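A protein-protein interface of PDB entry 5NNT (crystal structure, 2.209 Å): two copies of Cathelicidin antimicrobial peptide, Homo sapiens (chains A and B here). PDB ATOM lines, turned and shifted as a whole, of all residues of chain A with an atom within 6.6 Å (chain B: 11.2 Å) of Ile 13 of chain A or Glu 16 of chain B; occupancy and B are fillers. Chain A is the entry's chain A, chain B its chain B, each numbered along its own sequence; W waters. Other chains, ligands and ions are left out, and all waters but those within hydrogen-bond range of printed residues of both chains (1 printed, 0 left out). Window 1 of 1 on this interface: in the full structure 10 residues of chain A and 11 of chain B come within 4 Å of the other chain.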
ATOM      1  N   LYS A   8      29.431  25.581  -1.520  1.00  0.00           N
ATOM      2  CA  LYS A   8      28.836  26.902  -1.729  1.00  0.00           C
ATOM      3  C   LYS A   8      27.791  26.869  -2.836  1.00  0.00           C
ATOM      4  O   LYS A   8      26.733  27.508  -2.721  1.00  0.00           O
ATOM      5  CB  LYS A   8      29.933  27.916  -2.054  1.00  0.00           C
ATOM      6  CG  LYS A   8      30.967  28.074  -0.951  1.00  0.00           C
ATOM      7  CD  LYS A   8      30.910  29.451  -0.312  1.00  0.00           C
ATOM      8  CE  LYS A   8      31.604  29.458   1.041  1.00  0.00           C
ATOM      9  NZ  LYS A   8      31.993  30.829   1.470  1.00  0.00           N
ATOM     10  N   SER A   9      28.061  26.130  -3.913  1.00  0.00           N
ATOM     11  CA  SER A   9      27.096  26.017  -5.001  1.00  0.00           C
ATOM     12  C   SER A   9      25.847  25.266  -4.549  1.00  0.00           C
ATOM     13  O   SER A   9      24.718  25.684  -4.843  1.00  0.00           O
ATOM     14  CB  SER A   9      27.747  25.313  -6.192  1.00  0.00           C
ATOM     15  OG  SER A   9      28.603  26.197  -6.896  1.00  0.00           O
ATOM     16  N   LYS A  10      26.031  24.163  -3.821  1.00  0.00           N
ATOM     17  CA  LYS A  10      24.886  23.413  -3.320  1.00  0.00           C
ATOM     18  C   LYS A  10      24.058  24.266  -2.373  1.00  0.00           C
ATOM     19  O   LYS A  10      22.823  24.210  -2.391  1.00  0.00           O
ATOM     20  CB  LYS A  10      25.357  22.142  -2.612  1.00  0.00           C
ATOM     21  CG  LYS A  10      25.800  21.021  -3.544  1.00  0.00           C
ATOM     22  CD  LYS A  10      26.063  19.729  -2.779  1.00  0.00           C
ATOM     23  CE  LYS A  10      27.109  19.915  -1.691  1.00  0.00           C
ATOM     24  NZ  LYS A  10      27.534  18.624  -1.085  1.00  0.00           N
ATOM     25  N   GLU A  11      24.723  25.072  -1.544  1.00  0.00           N
ATOM     26  CA  GLU A  11      24.002  25.984  -0.665  1.00  0.00           C
ATOM     27  C   GLU A  11      23.183  26.982  -1.467  1.00  0.00           C
ATOM     28  O   GLU A  11      21.980  27.137  -1.237  1.00  0.00           O
ATOM     29  CB  GLU A  11      24.978  26.712   0.260  1.00  0.00           C
ATOM     30  CG  GLU A  11      25.335  25.930   1.509  1.00  0.00           C
ATOM     31  CD  GLU A  11      26.152  26.746   2.491  1.00  0.00           C
ATOM     32  OE1 GLU A  11      25.876  27.957   2.630  1.00  0.00           O
ATOM     33  OE2 GLU A  11      27.069  26.179   3.121  1.00  0.00           O
ATOM     34  N   LYS A  12      23.816  27.670  -2.423  1.00  0.00           N
ATOM     35  CA  LYS A  12      23.093  28.651  -3.231  1.00  0.00           C
ATOM     36  C   LYS A  12      21.858  28.031  -3.880  1.00  0.00           C
ATOM     37  O   LYS A  12      20.745  28.563  -3.763  1.00  0.00           O
ATOM     38  CB  LYS A  12      24.029  29.244  -4.287  1.00  0.00           C
ATOM     39  CG  LYS A  12      24.783  30.470  -3.796  1.00  0.00           C
ATOM     40  CD  LYS A  12      26.143  30.627  -4.464  1.00  0.00           C
ATOM     41  CE  LYS A  12      26.976  31.688  -3.756  1.00  0.00           C
ATOM     42  NZ  LYS A  12      28.142  32.139  -4.561  1.00  0.00           N
ATOM     43  N   ILE A  13      22.035  26.900  -4.568  1.00  0.00           N
ATOM     44  CA  ILE A  13      20.896  26.222  -5.184  1.00  0.00           C
ATOM     45  C   ILE A  13      19.819  25.944  -4.139  1.00  0.00           C
ATOM     46  O   ILE A  13      18.636  26.248  -4.343  1.00  0.00           O
ATOM     47  CB  ILE A  13      21.354  24.934  -5.894  1.00  0.00           C
ATOM     48  CG1 ILE A  13      22.187  25.289  -7.128  1.00  0.00           C
ATOM     49  CG2 ILE A  13      20.150  24.074  -6.293  1.00  0.00           C
ATOM     50  CD1 ILE A  13      22.927  24.116  -7.742  1.00  0.00           C
ATOM     51  N   GLY A  14      20.218  25.356  -3.008  1.00  0.00           N
ATOM     52  CA  GLY A  14      19.256  25.066  -1.956  1.00  0.00           C
ATOM     53  C   GLY A  14      18.450  26.284  -1.549  1.00  0.00           C
ATOM     54  O   GLY A  14      17.228  26.222  -1.422  1.00  0.00           O
ATOM     55  N   LYS A  15      19.131  27.410  -1.339  1.00  0.00           N
ATOM     56  CA  LYS A  15      18.445  28.621  -0.901  1.00  0.00           C
ATOM     57  C   LYS A  15      17.455  29.102  -1.951  1.00  0.00           C
ATOM     58  O   LYS A  15      16.293  29.383  -1.638  1.00  0.00           O
ATOM     59  CB  LYS A  15      19.455  29.721  -0.585  1.00  0.00           C
ATOM     60  CG  LYS A  15      20.113  29.570   0.760  1.00  0.00           C
ATOM     61  CD  LYS A  15      20.996  30.761   1.055  1.00  0.00           C
ATOM     62  CE  LYS A  15      21.918  30.482   2.213  1.00  0.00           C
ATOM     63  NZ  LYS A  15      23.157  31.305   2.169  1.00  0.00           N
ATOM     64  N   GLU A  16      17.904  29.231  -3.201  1.00  0.00           N
ATOM     65  CA  GLU A  16      16.998  29.702  -4.244  1.00  0.00           C
ATOM     66  C   GLU A  16      15.773  28.799  -4.357  1.00  0.00           C
ATOM     67  O   GLU A  16      14.640  29.285  -4.498  1.00  0.00           O
ATOM     68  CB  GLU A  16      17.741  29.783  -5.578  1.00  0.00           C
ATOM     69  CG  GLU A  16      18.925  30.728  -5.559  1.00  0.00           C
ATOM     70  CD  GLU A  16      18.530  32.145  -5.197  1.00  0.00           C
ATOM     71  OE1 GLU A  16      17.533  32.647  -5.753  1.00  0.00           O
ATOM     72  OE2 GLU A  16      19.238  32.769  -4.383  1.00  0.00           O
ATOM     73  N   PHE A  17      15.973  27.481  -4.268  1.00  0.00           N
ATOM     74  CA  PHE A  17      14.845  26.559  -4.350  1.00  0.00           C
ATOM     75  C   PHE A  17      13.902  26.736  -3.162  1.00  0.00           C
ATOM     76  O   PHE A  17      12.677  26.790  -3.332  1.00  0.00           O
ATOM     77  CB  PHE A  17      15.348  25.120  -4.425  1.00  0.00           C
ATOM     78  CG  PHE A  17      14.255  24.108  -4.599  1.00  0.00           C
ATOM     79  CD1 PHE A  17      13.885  23.693  -5.869  1.00  0.00           C
ATOM     80  CD2 PHE A  17      13.591  23.577  -3.506  1.00  0.00           C
ATOM     81  CE1 PHE A  17      12.881  22.765  -6.044  1.00  0.00           C
ATOM     82  CE2 PHE A  17      12.582  22.649  -3.675  1.00  0.00           C
ATOM     83  CZ  PHE A  17      12.229  22.242  -4.946  1.00  0.00           C
ATOM     84  N   LYS A  18      14.456  26.839  -1.951  1.00  0.00           N
ATOM     85  CA  LYS A  18      13.608  27.025  -0.776  1.00  0.00           C
ATOM     86  C   LYS A  18      12.784  28.294  -0.884  1.00  0.00           C
ATOM     87  O   LYS A  18      11.668  28.355  -0.357  1.00  0.00           O
ATOM     88  CB  LYS A  18      14.445  27.096   0.502  1.00  0.00           C
ATOM     89  CG  LYS A  18      14.804  25.769   1.143  1.00  0.00           C
ATOM     90  CD  LYS A  18      15.570  26.019   2.437  1.00  0.00           C
ATOM     91  CE  LYS A  18      15.761  24.750   3.246  1.00  0.00           C
ATOM     92  NZ  LYS A  18      17.156  24.237   3.168  1.00  0.00           N
ATOM     93  N   LEU B   1      10.672  26.598 -16.689  1.00  0.00           N
ATOM     94  CA  LEU B   1      10.103  25.556 -15.788  1.00  0.00           C
ATOM     95  C   LEU B   1       8.787  26.030 -15.187  1.00  0.00           C
ATOM     96  O   LEU B   1       7.811  25.288 -15.146  1.00  0.00           O
ATOM     97  CB  LEU B   1      11.087  25.212 -14.667  1.00  0.00           C
ATOM     98  CG  LEU B   1      10.678  24.078 -13.720  1.00  0.00           C
ATOM     99  CD1 LEU B   1      10.390  22.788 -14.483  1.00  0.00           C
ATOM    100  CD2 LEU B   1      11.740  23.854 -12.656  1.00  0.00           C
ATOM    101  N   LEU B   2       8.772  27.278 -14.724  1.00  0.00           N
ATOM    102  CA  LEU B   2       7.623  27.813 -14.004  1.00  0.00           C
ATOM    103  C   LEU B   2       7.070  29.023 -14.742  1.00  0.00           C
ATOM    104  O   LEU B   2       6.812  30.065 -14.132  1.00  0.00           O
ATOM    105  CB  LEU B   2       8.020  28.197 -12.579  1.00  0.00           C
ATOM    106  CG  LEU B   2       8.582  27.059 -11.725  1.00  0.00           C
ATOM    107  CD1 LEU B   2       9.649  27.608 -10.786  1.00  0.00           C
ATOM    108  CD2 LEU B   2       7.501  26.316 -10.952  1.00  0.00           C
ATOM    109  N   PHE B   6      10.068  33.730 -11.304  1.00  0.00           N
ATOM    110  CA  PHE B   6      11.345  33.324 -10.713  1.00  0.00           C
ATOM    111  C   PHE B   6      12.454  33.287 -11.765  1.00  0.00           C
ATOM    112  O   PHE B   6      13.232  32.335 -11.855  1.00  0.00           O
ATOM    113  CB  PHE B   6      11.207  31.979 -10.001  1.00  0.00           C
ATOM    114  CG  PHE B   6       9.984  31.882  -9.135  1.00  0.00           C
ATOM    115  CD1 PHE B   6       9.959  32.478  -7.885  1.00  0.00           C
ATOM    116  CD2 PHE B   6       8.856  31.208  -9.574  1.00  0.00           C
ATOM    117  CE1 PHE B   6       8.836  32.396  -7.084  1.00  0.00           C
ATOM    118  CE2 PHE B   6       7.729  31.126  -8.779  1.00  0.00           C
ATOM    119  CZ  PHE B   6       7.720  31.721  -7.531  1.00  0.00           C
ATOM    120  N   ARG B   7      12.525  34.354 -12.559  1.00  0.00           N
ATOM    121  CA  ARG B   7      13.552  34.461 -13.589  1.00  0.00           C
ATOM    122  C   ARG B   7      14.946  34.450 -12.971  1.00  0.00           C
ATOM    123  O   ARG B   7      15.799  33.630 -13.334  1.00  0.00           O
ATOM    124  CB  ARG B   7      13.324  35.741 -14.394  1.00  0.00           C
ATOM    125  CG  ARG B   7      13.970  35.777 -15.768  1.00  0.00           C
ATOM    126  CD  ARG B   7      13.643  37.087 -16.472  1.00  0.00           C
ATOM    127  NE  ARG B   7      13.929  37.042 -17.907  1.00  0.00           N
ATOM    128  CZ  ARG B   7      13.012  36.919 -18.867  1.00  0.00           C
ATOM    129  NH1 ARG B   7      11.716  36.830 -18.575  1.00  0.00           N
ATOM    130  NH2 ARG B   7      13.394  36.890 -20.136  1.00  0.00           N
ATOM    131  N   LYS B   8      15.185  35.350 -12.014  1.00  0.00           N
ATOM    132  CA  LYS B   8      16.502  35.461 -11.395  1.00  0.00           C
ATOM    133  C   LYS B   8      16.881  34.189 -10.648  1.00  0.00           C
ATOM    134  O   LYS B   8      18.024  33.727 -10.743  1.00  0.00           O
ATOM    135  CB  LYS B   8      16.528  36.666 -10.457  1.00  0.00           C
ATOM    136  CG  LYS B   8      17.770  36.753  -9.581  1.00  0.00           C
ATOM    137  CD  LYS B   8      17.755  37.992  -8.702  1.00  0.00           C
ATOM    138  CE  LYS B   8      16.713  37.900  -7.593  1.00  0.00           C
ATOM    139  NZ  LYS B   8      17.084  36.895  -6.559  1.00  0.00           N
ATOM    140  N   SER B   9      15.949  33.613  -9.886  1.00  0.00           N
ATOM    141  CA  SER B   9      16.266  32.403  -9.132  1.00  0.00           C
ATOM    142  C   SER B   9      16.603  31.244 -10.061  1.00  0.00           C
ATOM    143  O   SER B   9      17.571  30.512  -9.824  1.00  0.00           O
ATOM    144  CB  SER B   9      15.104  32.033  -8.212  1.00  0.00           C
ATOM    145  OG  SER B   9      15.104  32.850  -7.059  1.00  0.00           O
ATOM    146  N   LYS B  10      15.816  31.058 -11.123  1.00  0.00           N
ATOM    147  CA  LYS B  10      16.106  29.989 -12.073  1.00  0.00           C
ATOM    148  C   LYS B  10      17.443  30.217 -12.769  1.00  0.00           C
ATOM    149  O   LYS B  10      18.185  29.261 -13.022  1.00  0.00           O
ATOM    150  CB  LYS B  10      14.974  29.865 -13.092  1.00  0.00           C
ATOM    151  CG  LYS B  10      13.753  29.144 -12.545  1.00  0.00           C
ATOM    152  CD  LYS B  10      12.728  28.850 -13.628  1.00  0.00           C
ATOM    153  CE  LYS B  10      12.240  30.123 -14.306  1.00  0.00           C
ATOM    154  NZ  LYS B  10      11.083  29.863 -15.209  1.00  0.00           N
ATOM    155  N   GLU B  11      17.765  31.470 -13.100  1.00  0.00           N
ATOM    156  CA  GLU B  11      19.077  31.752 -13.680  1.00  0.00           C
ATOM    157  C   GLU B  11      20.190  31.392 -12.704  1.00  0.00           C
ATOM    158  O   GLU B  11      21.204  30.800 -13.095  1.00  0.00           O
ATOM    159  CB  GLU B  11      19.175  33.224 -14.083  1.00  0.00           C
ATOM    160  CG  GLU B  11      18.595  33.530 -15.458  1.00  0.00           C
ATOM    161  CD  GLU B  11      18.866  34.954 -15.905  1.00  0.00           C
ATOM    162  OE1 GLU B  11      19.972  35.467 -15.631  1.00  0.00           O
ATOM    163  OE2 GLU B  11      17.973  35.560 -16.534  1.00  0.00           O
ATOM    164  N   LYS B  12      20.020  31.743 -11.428  1.00  0.00           N
ATOM    165  CA  LYS B  12      21.001  31.390 -10.406  1.00  0.00           C
ATOM    166  C   LYS B  12      21.202  29.880 -10.346  1.00  0.00           C
ATOM    167  O   LYS B  12      22.331  29.380 -10.444  1.00  0.00           O
ATOM    168  CB  LYS B  12      20.541  31.935  -9.051  1.00  0.00           C
ATOM    169  CG  LYS B  12      21.529  31.748  -7.907  1.00  0.00           C
ATOM    170  CD  LYS B  12      22.778  32.588  -8.094  1.00  0.00           C
ATOM    171  CE  LYS B  12      23.653  32.547  -6.854  1.00  0.00           C
ATOM    172  NZ  LYS B  12      25.064  32.899  -7.159  1.00  0.00           N
ATOM    173  N   ILE B  13      20.106  29.134 -10.175  1.00  0.00           N
ATOM    174  CA  ILE B  13      20.190  27.677 -10.101  1.00  0.00           C
ATOM    175  C   ILE B  13      20.900  27.132 -11.332  1.00  0.00           C
ATOM    176  O   ILE B  13      21.861  26.361 -11.232  1.00  0.00           O
ATOM    177  CB  ILE B  13      18.783  27.068  -9.951  1.00  0.00           C
ATOM    178  CG1 ILE B  13      18.194  27.406  -8.581  1.00  0.00           C
ATOM    179  CG2 ILE B  13      18.824  25.547 -10.155  1.00  0.00           C
ATOM    180  CD1 ILE B  13      16.709  27.099  -8.462  1.00  0.00           C
ATOM    181  N   GLY B  14      20.438  27.541 -12.515  1.00  0.00           N
ATOM    182  CA  GLY B  14      21.061  27.082 -13.746  1.00  0.00           C
ATOM    183  C   GLY B  14      22.554  27.315 -13.760  1.00  0.00           C
ATOM    184  O   GLY B  14      23.332  26.435 -14.134  1.00  0.00           O
ATOM    185  N   LYS B  15      22.982  28.516 -13.365  1.00  0.00           N
ATOM    186  CA  LYS B  15      24.400  28.852 -13.396  1.00  0.00           C
ATOM    187  C   LYS B  15      25.199  27.970 -12.440  1.00  0.00           C
ATOM    188  O   LYS B  15      26.198  27.356 -12.835  1.00  0.00           O
ATOM    189  CB  LYS B  15      24.588  30.324 -13.045  1.00  0.00           C
ATOM    190  CG  LYS B  15      24.226  31.269 -14.167  1.00  0.00           C
ATOM    191  CD  LYS B  15      24.525  32.692 -13.766  1.00  0.00           C
ATOM    192  CE  LYS B  15      23.827  33.675 -14.668  1.00  0.00           C
ATOM    193  NZ  LYS B  15      23.574  34.953 -13.950  1.00  0.00           N
ATOM    194  N   GLU B  16      24.775  27.901 -11.174  1.00  0.00           N
ATOM    195  CA  GLU B  16      25.507  27.076 -10.215  1.00  0.00           C
ATOM    196  C   GLU B  16      25.580  25.634 -10.696  1.00  0.00           C
ATOM    197  O   GLU B  16      26.623  24.978 -10.571  1.00  0.00           O
ATOM    198  CB  GLU B  16      24.852  27.153  -8.834  1.00  0.00           C
ATOM    199  CG  GLU B  16      24.805  28.562  -8.245  1.00  0.00           C
ATOM    200  CD  GLU B  16      26.181  29.186  -8.098  1.00  0.00           C
ATOM    201  OE1 GLU B  16      27.083  28.525  -7.538  1.00  0.00           O
ATOM    202  OE2 GLU B  16      26.371  30.327  -8.569  1.00  0.00           O
ATOM    203  N   PHE B  17      24.486  25.130 -11.269  1.00  0.00           N
ATOM    204  CA  PHE B  17      24.480  23.771 -11.795  1.00  0.00           C
ATOM    205  C   PHE B  17      25.483  23.621 -12.933  1.00  0.00           C
ATOM    206  O   PHE B  17      26.232  22.640 -12.987  1.00  0.00           O
ATOM    207  CB  PHE B  17      23.071  23.403 -12.264  1.00  0.00           C
ATOM    208  CG  PHE B  17      22.959  22.010 -12.817  1.00  0.00           C
ATOM    209  CD1 PHE B  17      22.839  20.916 -11.975  1.00  0.00           C
ATOM    210  CD2 PHE B  17      22.965  21.796 -14.187  1.00  0.00           C
ATOM    211  CE1 PHE B  17      22.733  19.637 -12.490  1.00  0.00           C
ATOM    212  CE2 PHE B  17      22.857  20.520 -14.705  1.00  0.00           C
ATOM    213  CZ  PHE B  17      22.741  19.441 -13.856  1.00  0.00           C
ATOM    214  N   LYS B  18      25.510  24.589 -13.851  1.00  0.00           N
ATOM    215  CA  LYS B  18      26.450  24.541 -14.966  1.00  0.00           C
ATOM    216  C   LYS B  18      27.891  24.575 -14.479  1.00  0.00           C
ATOM    217  O   LYS B  18      28.778  23.984 -15.106  1.00  0.00           O
ATOM    218  CB  LYS B  18      26.181  25.712 -15.910  1.00  0.00           C
ATOM    219  CG  LYS B  18      25.047  25.469 -16.892  1.00  0.00           C
ATOM    220  CD  LYS B  18      24.847  26.668 -17.806  1.00  0.00           C
ATOM    221  CE  LYS B  18      23.866  26.362 -18.922  1.00  0.00           C
ATOM    222  NZ  LYS B  18      24.435  26.693 -20.258  1.00  0.00           N
ATOM    223  N   ARG B  19      28.135  25.230 -13.345  1.00  0.00           N
ATOM    224  CA  ARG B  19      29.487  25.305 -12.806  1.00  0.00           C
ATOM    225  C   ARG B  19      29.881  23.990 -12.144  1.00  0.00           C
ATOM    226  O   ARG B  19      30.999  23.498 -12.349  1.00  0.00           O
ATOM    227  CB  ARG B  19      29.574  26.463 -11.815  1.00  0.00           C
ATOM    228  CG  ARG B  19      30.919  26.647 -11.146  1.00  0.00           C
ATOM    229  CD  ARG B  19      30.834  27.757 -10.112  1.00  0.00           C
ATOM    230  NE  ARG B  19      30.886  29.085 -10.719  1.00  0.00           N
ATOM    231  CZ  ARG B  19      30.308  30.173 -10.212  1.00  0.00           C
ATOM    232  NH1 ARG B  19      29.609  30.109  -9.086  1.00  0.00           N
ATOM    233  NH2 ARG B  19      30.423  31.333 -10.842  1.00  0.00           N
ATOM    234  N   ILE B  20      28.972  23.403 -11.358  1.00  0.00           N
ATOM    235  CA  ILE B  20      29.204  22.058 -10.829  1.00  0.00           C
ATOM    236  C   ILE B  20      29.525  21.093 -11.964  1.00  0.00           C
ATOM    237  O   ILE B  20      30.529  20.367 -11.928  1.00  0.00           O
ATOM    238  CB  ILE B  20      27.985  21.588 -10.014  1.00  0.00           C
ATOM    239  CG1 ILE B  20      27.861  22.417  -8.731  1.00  0.00           C
ATOM    240  CG2 ILE B  20      28.063  20.076  -9.728  1.00  0.00           C
ATOM    241  CD1 ILE B  20      26.651  22.070  -7.878  1.00  0.00           C
ATOM    242  N   VAL B  21      28.694  21.098 -13.006  1.00  0.00           N
ATOM    243  CA  VAL B  21      28.891  20.177 -14.119  1.00  0.00           C
ATOM    244  C   VAL B  21      30.232  20.442 -14.786  1.00  0.00           C
ATOM    245  O   VAL B  21      30.941  19.508 -15.172  1.00  0.00           O
ATOM    246  CB  VAL B  21      27.724  20.274 -15.119  1.00  0.00           C
ATOM    247  CG1 VAL B  21      28.053  19.518 -16.414  1.00  0.00           C
ATOM    248  CG2 VAL B  21      26.454  19.739 -14.495  1.00  0.00           C
ATOM    249  N   GLN B  22      30.582  21.716 -14.970  1.00  0.00           N
ATOM    250  CA  GLN B  22      31.859  22.028 -15.601  1.00  0.00           C
ATOM    251  C   GLN B  22      33.023  21.475 -14.793  1.00  0.00           C
ATOM    252  O   GLN B  22      33.957  20.891 -15.358  1.00  0.00           O
ATOM    253  CB  GLN B  22      32.013  23.537 -15.783  1.00  0.00           C
ATOM    254  CG  GLN B  22      33.112  23.889 -16.770  1.00  0.00           C
ATOM    255  CD  GLN B  22      32.901  23.250 -18.125  1.00  0.00           C
ATOM    256  OE1 GLN B  22      31.809  23.309 -18.688  1.00  0.00           O
ATOM    257  NE2 GLN B  22      33.927  22.569 -18.623  1.00  0.00           N
ATOM    258  N   ARG B  23      32.988  21.637 -13.469  1.00  0.00           N
ATOM    259  CA  ARG B  23      34.080  21.117 -12.654  1.00  0.00           C
ATOM    260  C   ARG B  23      34.139  19.596 -12.731  1.00  0.00           C
ATOM    261  O   ARG B  23      35.226  19.015 -12.847  1.00  0.00           O
ATOM    262  CB  ARG B  23      33.927  21.580 -11.207  1.00  0.00           C
ATOM    263  CG  ARG B  23      33.819  23.082 -11.062  1.00  0.00           C
ATOM    264  CD  ARG B  23      34.698  23.617  -9.946  1.00  0.00           C
ATOM    265  NE  ARG B  23      34.380  25.008  -9.636  1.00  0.00           N
ATOM    266  CZ  ARG B  23      34.682  26.042 -10.417  1.00  0.00           C
ATOM    267  NH1 ARG B  23      35.316  25.852 -11.566  1.00  0.00           N
ATOM    268  NH2 ARG B  23      34.349  27.270 -10.047  1.00  0.00           N
ATOM    269  N   ILE B  24      32.981  18.935 -12.683  1.00  0.00           N
ATOM    270  CA  ILE B  24      32.955  17.480 -12.827  1.00  0.00           C
ATOM    271  C   ILE B  24      33.585  17.071 -14.152  1.00  0.00           C
ATOM    272  O   ILE B  24      34.429  16.167 -14.207  1.00  0.00           O
ATOM    273  CB  ILE B  24      31.513  16.958 -12.691  1.00  0.00           C
ATOM    274  CG1 ILE B  24      31.020  17.168 -11.258  1.00  0.00           C
ATOM    275  CG2 ILE B  24      31.436  15.477 -13.070  1.00  0.00           C
ATOM    276  CD1 ILE B  24      29.565  16.805 -11.037  1.00  0.00           C
ATOM    277  N   LYS B  25      33.199  17.741 -15.243  1.00  0.00           N
ATOM    278  CA  LYS B  25      33.795  17.435 -16.539  1.00  0.00           C
ATOM    279  C   LYS B  25      35.304  17.606 -16.504  1.00  0.00           C
ATOM    280  O   LYS B  25      36.037  16.780 -17.055  1.00  0.00           O
ATOM    281  CB  LYS B  25      33.201  18.315 -17.639  1.00  0.00           C
ATOM    282  CG  LYS B  25      32.098  17.646 -18.449  1.00  0.00           C
ATOM    283  CD  LYS B  25      31.098  18.656 -18.995  1.00  0.00           C
ATOM    284  CE  LYS B  25      31.004  18.576 -20.517  1.00  0.00           C
ATOM    285  NZ  LYS B  25      32.129  19.286 -21.195  1.00  0.00           N
HETATM  286  O   HOH W   1      29.594  29.321  -6.392  1.00  0.00           O
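OG of Ser 9 of chain A lies within hydrogen-bond range of OE1 of Glu 16 of chain B (2.9 Å). The side-chain hydroxyl of Ser 9 of chain B is in hydrogen-bond range of the side-chain carboxylate of Glu 16 of chain A (2.8 Å).
The side-chain amino group (NZ) of Lys 12 of chain B is in salt-bridge range of the side-chain carboxylate (OE2) of Glu 16 of chain B (3.2 Å). The side-chain carboxylate (OE2) of Glu 16 of chain B is in salt-bridge range of the guanidinium group (NH1) of Arg 19 of chain B, 3.3 Å away.
Of the 22 printed residues of chain B, 6 touch a printed residue of chain A. Printed residues of chain B that touch a printed residue of chain A: Ser 9, Lys 12, Ile 13, Glu 16, Phe 17 and Ile 20. Hydrophobic or aromatic side chains of chain B that line the printed part of chain A: Ile 13 and Ile 20. Along chain A the printed residues that touch a printed residue of chain B span positions 9 to 16. Among the printed residues, 9 pairs touch across the chains.
Water W1 lies within hydrogen-bond range of the guanidinium group of Arg 19 of chain B (2.8 Å), the side-chain carboxylate of Glu 16 of chain B (2.9 Å) and the side-chain hydroxyl of Ser 9 of chain A (3.3 Å).
CB of Ser 9 of chain A touches CD1 of Ile 20 of chain B, at 3.8 Å. Lys 12 of chain B touches Lys 12 of chain A. OE1 of Glu 16 of chain B touches CD of Lys 12 of chain A (3.8 Å). CB of Glu 16 of chain B touches CG1 of Ile 13 of chain A, at 3.7 Å. Ile 13 of chain A touches Phe 17 of chain B (CD1 to N, 3.99 Å). Lys 12 of chain B touches Glu 16 of chain A (CG to CG, 3.7 Å). CG1 of Ile 13 of chain B touches CB of Glu 16 of chain A, at 3.9 Å.
Of chain B, only Lys 12 and Glu 16 come within 4 Å of Lys 12 of chain A. Gly 14 of chain A touches none of the printed residues of chain B. Glu 16 of chain A touches just these residues of chain B: Ser 9, Lys 12 and Ile 13. Printed residues of chain A within 4 Å of Ser 9 of chain B: Glu 16. Of the printed residues of chain A, Lys 12 of chain B touches Lys 12 (3.7 Å) and Glu 16 (3.7 Å). Glu 16 of chain B touches just these residues of chain A: Ser 9, Lys 12 and Ile 13. Printed residues of chain A within 4 Å of Phe 17 of chain B: Ile 13 (3.99 Å). Printed residues of chain A within 4 Å of Ile 20 of chain B: Ser 9 (3.8 Å). The nearest printed residue of chain A that does not touch Glu 16 of chain B is Lys 8 of chain A (4.9 Å). The nearest printed residue of chain A that does not touch Ile 13 of chain B is Ile 13 of chain A (4.3 Å).
Ser 9 of chain A touches Glu 16 of chain B, and with the chains exchanged Glu 16 of chain A touches Ser 9 of chain B. Lys 12 of chain B touches its own counterpart, Lys 12 of chain A. Ile 13 of chain A touches Glu 16 of chain B, and with the chains exchanged Glu 16 of chain A touches Ile 13 of chain B. Ile 13 of chain A touches Phe 17 of chain B, but with the chains exchanged Phe 17 of chain A does not touch Ile 13 of chain B (4.3 Å). Of the 9 pairs that touch across the chains among the printed residues, 7 have their exchanged pair printed and touching as well.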
